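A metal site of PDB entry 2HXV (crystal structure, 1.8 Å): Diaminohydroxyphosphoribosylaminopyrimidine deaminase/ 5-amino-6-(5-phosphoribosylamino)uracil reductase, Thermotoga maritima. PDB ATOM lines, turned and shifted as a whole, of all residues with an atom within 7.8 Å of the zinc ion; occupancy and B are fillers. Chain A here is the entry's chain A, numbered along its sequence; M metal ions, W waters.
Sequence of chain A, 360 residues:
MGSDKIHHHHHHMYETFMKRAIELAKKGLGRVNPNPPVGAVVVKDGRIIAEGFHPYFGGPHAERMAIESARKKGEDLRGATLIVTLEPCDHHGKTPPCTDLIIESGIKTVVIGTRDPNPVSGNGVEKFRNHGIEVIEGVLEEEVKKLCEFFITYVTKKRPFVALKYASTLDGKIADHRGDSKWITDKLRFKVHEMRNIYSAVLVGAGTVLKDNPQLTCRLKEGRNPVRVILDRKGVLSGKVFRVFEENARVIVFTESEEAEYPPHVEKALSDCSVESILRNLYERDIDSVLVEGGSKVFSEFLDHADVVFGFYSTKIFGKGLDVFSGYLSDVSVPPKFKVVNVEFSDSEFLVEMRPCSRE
Glu 63 touches the zinc ion (OE2 to ZN, 3.9 Å).
Within 4 Å of the zinc ion: His 61, Glu 63, Cys 89 and Cys 98.
The nearest printed residue that does not touch the zinc ion is Pro 88 (4.9 Å).
The backbone NH (N) of Thr 99 sits at hydrogen-bond distance from the backbone carbonyl oxygen (O) of Cys 89 (3.1 Å).
The side-chain sulfur of Cys 98 sits close to the side-chain carboxylate of Glu 63 (3.7 Å).
The zinc ion is bound by water W1 (2.1 Å), ND1 of His 61 (2.1 Å), SG of Cys 98 (2.2 Å) and SG of Cys 89 (2.3 Å).
The zinc ion has four donor atoms within binding distance.
Water W1 lies within hydrogen-bond range of the side-chain carboxylate (OE2) of Glu 63 (2.6 Å) and the backbone NH (N) of Cys 89 (3.0 Å).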
ATOM      1  N   VAL A  38      30.865  -8.529  27.201  1.00  0.00           N
ATOM      2  CA  VAL A  38      31.543  -8.555  25.890  1.00  0.00           C
ATOM      3  C   VAL A  38      31.521  -7.194  25.293  1.00  0.00           C
ATOM      4  O   VAL A  38      30.514  -6.449  25.371  1.00  0.00           O
ATOM      5  CB  VAL A  38      30.900  -9.539  24.896  1.00  0.00           C
ATOM      6  CG1 VAL A  38      31.717  -9.622  23.617  1.00  0.00           C
ATOM      7  CG2 VAL A  38      30.778 -10.892  25.552  1.00  0.00           C
ATOM      8  N   HIS A  54      27.586  -5.986  25.232  1.00  0.00           N
ATOM      9  CA  HIS A  54      26.445  -6.809  25.690  1.00  0.00           C
ATOM     10  C   HIS A  54      25.794  -6.111  26.906  1.00  0.00           C
ATOM     11  O   HIS A  54      26.446  -5.912  27.924  1.00  0.00           O
ATOM     12  CB  HIS A  54      26.923  -8.220  25.972  1.00  0.00           C
ATOM     13  CG  HIS A  54      25.855  -9.234  26.231  1.00  0.00           C
ATOM     14  ND1 HIS A  54      24.742  -9.375  25.438  1.00  0.00           N
ATOM     15  CD2 HIS A  54      25.780 -10.220  27.163  1.00  0.00           C
ATOM     16  CE1 HIS A  54      24.003 -10.389  25.899  1.00  0.00           C
ATOM     17  NE2 HIS A  54      24.633 -10.929  26.928  1.00  0.00           N
ATOM     18  N   GLY A  59      20.271 -10.019  26.103  1.00  0.00           N
ATOM     19  CA  GLY A  59      20.233  -8.906  25.186  1.00  0.00           C
ATOM     20  C   GLY A  59      21.099  -9.113  23.962  1.00  0.00           C
ATOM     21  O   GLY A  59      21.702 -10.168  23.771  1.00  0.00           O
ATOM     22  N   PRO A  60      21.165  -8.090  23.080  1.00  0.00           N
ATOM     23  CA  PRO A  60      21.905  -8.237  21.848  1.00  0.00           C
ATOM     24  C   PRO A  60      23.352  -8.429  22.133  1.00  0.00           C
ATOM     25  O   PRO A  60      23.846  -7.907  23.141  1.00  0.00           O
ATOM     26  CB  PRO A  60      21.730  -6.873  21.168  1.00  0.00           C
ATOM     27  CG  PRO A  60      20.689  -6.206  21.842  1.00  0.00           C
ATOM     28  CD  PRO A  60      20.500  -6.790  23.182  1.00  0.00           C
ATOM     29  N   HIS A  61      24.019  -9.196  21.282  1.00  0.00           N
ATOM     30  CA  HIS A  61      25.409  -9.440  21.452  1.00  0.00           C
ATOM     31  C   HIS A  61      26.156  -8.198  21.011  1.00  0.00           C
ATOM     32  O   HIS A  61      25.656  -7.425  20.195  1.00  0.00           O
ATOM     33  CB  HIS A  61      25.786 -10.691  20.718  1.00  0.00           C
ATOM     34  CG  HIS A  61      25.223 -11.907  21.369  1.00  0.00           C
ATOM     35  ND1 HIS A  61      25.529 -13.187  20.997  1.00  0.00           N
ATOM     36  CD2 HIS A  61      24.401 -12.027  22.456  1.00  0.00           C
ATOM     37  CE1 HIS A  61      24.919 -14.045  21.773  1.00  0.00           C
ATOM     38  NE2 HIS A  61      24.220 -13.371  22.681  1.00  0.00           N
ATOM     39  N   ALA A  62      27.316  -8.008  21.604  1.00  0.00           N
ATOM     40  CA  ALA A  62      28.117  -6.838  21.365  1.00  0.00           C
ATOM     41  C   ALA A  62      28.418  -6.657  19.866  1.00  0.00           C
ATOM     42  O   ALA A  62      28.411  -5.522  19.351  1.00  0.00           O
ATOM     43  CB  ALA A  62      29.354  -6.945  22.145  1.00  0.00           C
ATOM     44  N   GLU A  63      28.765  -7.763  19.205  1.00  0.00           N
ATOM     45  CA  GLU A  63      29.085  -7.725  17.782  1.00  0.00           C
ATOM     46  C   GLU A  63      27.910  -7.255  16.946  1.00  0.00           C
ATOM     47  O   GLU A  63      28.080  -6.448  15.991  1.00  0.00           O
ATOM     48  CB  GLU A  63      29.480  -9.122  17.299  1.00  0.00           C
ATOM     49  CG  GLU A  63      30.556  -9.760  18.027  1.00  0.00           C
ATOM     50  CD  GLU A  63      30.074 -10.688  19.077  1.00  0.00           C
ATOM     51  OE1 GLU A  63      29.464 -10.145  19.976  1.00  0.00           O
ATOM     52  OE2 GLU A  63      30.298 -11.904  19.010  1.00  0.00           O
ATOM     53  N   ARG A  64      26.703  -7.711  17.282  1.00  0.00           N
ATOM     54  CA  ARG A  64      25.533  -7.288  16.584  1.00  0.00           C
ATOM     55  C   ARG A  64      25.250  -5.823  16.799  1.00  0.00           C
ATOM     56  O   ARG A  64      24.938  -5.125  15.882  1.00  0.00           O
ATOM     57  CB  ARG A  64      24.311  -8.079  17.043  1.00  0.00           C
ATOM     58  CG  ARG A  64      23.054  -7.753  16.269  1.00  0.00           C
ATOM     59  CD  ARG A  64      21.947  -8.822  16.451  1.00  0.00           C
ATOM     60  NE  ARG A  64      22.258 -10.129  15.840  1.00  0.00           N
ATOM     61  CZ  ARG A  64      22.124 -10.447  14.547  1.00  0.00           C
ATOM     62  NH1 ARG A  64      21.712  -9.563  13.670  1.00  0.00           N
ATOM     63  NH2 ARG A  64      22.422 -11.663  14.129  1.00  0.00           N
ATOM     64  N   LEU A  86      35.423 -11.596  23.310  1.00  0.00           N
ATOM     65  CA  LEU A  86      35.145 -13.017  23.331  1.00  0.00           C
ATOM     66  C   LEU A  86      34.833 -13.535  21.933  1.00  0.00           C
ATOM     67  O   LEU A  86      34.197 -12.853  21.136  1.00  0.00           O
ATOM     68  CB  LEU A  86      33.909 -13.216  24.245  1.00  0.00           C
ATOM     69  CG  LEU A  86      33.540 -14.662  24.589  1.00  0.00           C
ATOM     70  CD1 LEU A  86      34.705 -15.307  25.331  1.00  0.00           C
ATOM     71  CD2 LEU A  86      32.257 -14.712  25.385  1.00  0.00           C
ATOM     72  N   GLU A  87      35.276 -14.754  21.628  1.00  0.00           N
ATOM     73  CA  GLU A  87      34.946 -15.413  20.394  1.00  0.00           C
ATOM     74  C   GLU A  87      33.478 -15.318  20.126  1.00  0.00           C
ATOM     75  O   GLU A  87      32.670 -15.707  20.995  1.00  0.00           O
ATOM     76  CB  GLU A  87      35.315 -16.899  20.511  1.00  0.00           C
ATOM     77  CG  GLU A  87      35.101 -17.705  19.270  1.00  0.00           C
ATOM     78  CD  GLU A  87      35.323 -19.204  19.518  1.00  0.00           C
ATOM     79  OE1 GLU A  87      35.529 -19.599  20.696  1.00  0.00           O
ATOM     80  OE2 GLU A  87      35.287 -19.975  18.548  1.00  0.00           O
ATOM     81  N   PRO A  88      33.113 -14.788  18.949  1.00  0.00           N
ATOM     82  CA  PRO A  88      31.716 -14.780  18.511  1.00  0.00           C
ATOM     83  C   PRO A  88      30.986 -16.139  18.485  1.00  0.00           C
ATOM     84  O   PRO A  88      31.580 -17.163  18.129  1.00  0.00           O
ATOM     85  CB  PRO A  88      31.777 -14.181  17.112  1.00  0.00           C
ATOM     86  CG  PRO A  88      32.977 -13.256  17.177  1.00  0.00           C
ATOM     87  CD  PRO A  88      33.977 -14.024  18.019  1.00  0.00           C
ATOM     88  N   CYS A  89      29.709 -16.087  18.824  1.00  0.00           N
ATOM     89  CA  CYS A  89      28.876 -17.295  18.937  1.00  0.00           C
ATOM     90  C   CYS A  89      28.595 -17.783  17.558  1.00  0.00           C
ATOM     91  O   CYS A  89      28.525 -17.013  16.610  1.00  0.00           O
ATOM     92  CB  CYS A  89      27.552 -17.029  19.646  1.00  0.00           C
ATOM     93  SG  CYS A  89      26.427 -15.887  18.851  1.00  0.00           S
ATOM     94  N   ASP A  90      28.437 -19.089  17.449  1.00  0.00           N
ATOM     95  CA  ASP A  90      28.064 -19.723  16.228  1.00  0.00           C
ATOM     96  C   ASP A  90      26.798 -20.559  16.496  1.00  0.00           C
ATOM     97  O   ASP A  90      26.631 -21.600  15.891  1.00  0.00           O
ATOM     98  CB  ASP A  90      29.219 -20.590  15.740  1.00  0.00           C
ATOM     99  CG  ASP A  90      29.050 -21.066  14.308  1.00  0.00           C
ATOM    100  OD1 ASP A  90      28.528 -20.286  13.462  1.00  0.00           O
ATOM    101  OD2 ASP A  90      29.439 -22.231  14.036  1.00  0.00           O
ATOM    102  N   HIS A  91      25.906 -20.115  17.371  1.00  0.00           N
ATOM    103  CA  HIS A  91      24.597 -20.757  17.496  1.00  0.00           C
ATOM    104  C   HIS A  91      23.431 -19.793  17.198  1.00  0.00           C
ATOM    105  O   HIS A  91      23.431 -18.625  17.619  1.00  0.00           O
ATOM    106  CB  HIS A  91      24.420 -21.361  18.890  1.00  0.00           C
ATOM    107  CG  HIS A  91      24.366 -20.332  19.976  1.00  0.00           C
ATOM    108  ND1 HIS A  91      25.495 -19.832  20.584  1.00  0.00           N
ATOM    109  CD2 HIS A  91      23.311 -19.690  20.546  1.00  0.00           C
ATOM    110  CE1 HIS A  91      25.146 -18.942  21.494  1.00  0.00           C
ATOM    111  NE2 HIS A  91      23.825 -18.830  21.485  1.00  0.00           N
ATOM    112  N   THR A  95      18.195 -14.825  17.315  1.00  0.00           N
ATOM    113  CA  THR A  95      18.741 -14.368  16.053  1.00  0.00           C
ATOM    114  C   THR A  95      19.724 -15.369  15.438  1.00  0.00           C
ATOM    115  O   THR A  95      20.193 -16.294  16.104  1.00  0.00           O
ATOM    116  CB  THR A  95      19.473 -13.029  16.238  1.00  0.00           C
ATOM    117  OG1 THR A  95      20.533 -13.167  17.203  1.00  0.00           O
ATOM    118  CG2 THR A  95      18.479 -11.958  16.718  1.00  0.00           C
ATOM    119  N   PRO A  96      20.063 -15.173  14.171  1.00  0.00           N
ATOM    120  CA  PRO A  96      21.185 -15.914  13.609  1.00  0.00           C
ATOM    121  C   PRO A  96      22.446 -15.663  14.423  1.00  0.00           C
ATOM    122  O   PRO A  96      22.535 -14.674  15.157  1.00  0.00           O
ATOM    123  CB  PRO A  96      21.331 -15.327  12.203  1.00  0.00           C
ATOM    124  CG  PRO A  96      20.003 -14.767  11.885  1.00  0.00           C
ATOM    125  CD  PRO A  96      19.445 -14.284  13.177  1.00  0.00           C
ATOM    126  N   PRO A  97      23.404 -16.590  14.342  1.00  0.00           N
ATOM    127  CA  PRO A  97      24.627 -16.384  15.118  1.00  0.00           C
ATOM    128  C   PRO A  97      25.440 -15.177  14.685  1.00  0.00           C
ATOM    129  O   PRO A  97      25.348 -14.737  13.574  1.00  0.00           O
ATOM    130  CB  PRO A  97      25.417 -17.652  14.862  1.00  0.00           C
ATOM    131  CG  PRO A  97      24.842 -18.264  13.659  1.00  0.00           C
ATOM    132  CD  PRO A  97      23.439 -17.826  13.561  1.00  0.00           C
ATOM    133  N   CYS A  98      26.301 -14.703  15.572  1.00  0.00           N
ATOM    134  CA  CYS A  98      27.173 -13.560  15.262  1.00  0.00           C
ATOM    135  C   CYS A  98      28.155 -13.929  14.167  1.00  0.00           C
ATOM    136  O   CYS A  98      28.512 -13.087  13.344  1.00  0.00           O
ATOM    137  CB  CYS A  98      27.891 -13.086  16.516  1.00  0.00           C
ATOM    138  SG  CYS A  98      26.826 -12.241  17.676  1.00  0.00           S
ATOM    139  N   THR A  99      28.572 -15.179  14.106  1.00  0.00           N
ATOM    140  CA  THR A  99      29.413 -15.591  13.001  1.00  0.00           C
ATOM    141  C   THR A  99      28.821 -15.252  11.638  1.00  0.00           C
ATOM    142  O   THR A  99      29.491 -14.595  10.805  1.00  0.00           O
ATOM    143  CB  THR A  99      29.670 -17.073  13.002  1.00  0.00           C
ATOM    144  OG1 THR A  99      28.411 -17.728  13.199  1.00  0.00           O
ATOM    145  CG2 THR A  99      30.624 -17.401  14.114  1.00  0.00           C
ATOM    146  N   LEU A 101      26.405 -13.070  10.890  1.00  0.00           N
ATOM    147  CA  LEU A 101      26.319 -11.624  10.758  1.00  0.00           C
ATOM    148  C   LEU A 101      27.651 -11.021  10.294  1.00  0.00           C
ATOM    149  O   LEU A 101      27.727 -10.190   9.383  1.00  0.00           O
ATOM    150  CB  LEU A 101      25.958 -11.043  12.109  1.00  0.00           C
ATOM    151  CG  LEU A 101      25.861  -9.509  12.129  1.00  0.00           C
ATOM    152  CD1 LEU A 101      24.893  -9.062  11.124  1.00  0.00           C
ATOM    153  CD2 LEU A 101      25.521  -9.022  13.539  1.00  0.00           C
ATOM    154  N   ILE A 102      28.722 -11.448  10.969  1.00  0.00           N
ATOM    155  CA  ILE A 102      30.068 -10.934  10.691  1.00  0.00           C
ATOM    156  C   ILE A 102      30.507 -11.287   9.270  1.00  0.00           C
ATOM    157  O   ILE A 102      30.966 -10.446   8.528  1.00  0.00           O
ATOM    158  CB  ILE A 102      31.094 -11.430  11.760  1.00  0.00           C
ATOM    159  CG1 ILE A 102      30.742 -10.799  13.106  1.00  0.00           C
ATOM    160  CG2 ILE A 102      32.538 -11.059  11.436  1.00  0.00           C
ATOM    161  CD1 ILE A 102      31.272 -11.548  14.291  1.00  0.00           C
ATOM    162  N   SER A 121      28.544 -22.547  22.425  1.00  0.00           N
ATOM    163  CA  SER A 121      28.837 -21.381  21.561  1.00  0.00           C
ATOM    164  C   SER A 121      29.368 -21.809  20.179  1.00  0.00           C
ATOM    165  O   SER A 121      29.310 -21.044  19.225  1.00  0.00           O
ATOM    166  CB  SER A 121      29.829 -20.439  22.254  1.00  0.00           C
ATOM    167  OG  SER A 121      31.102 -21.039  22.311  1.00  0.00           O
HETATM  168 ZN    ZN M   1      26.822 -13.676  19.368  1.00  0.00          ZN
HETATM  169  O   HOH W   1      28.735 -13.585  20.215  1.00  0.00           O
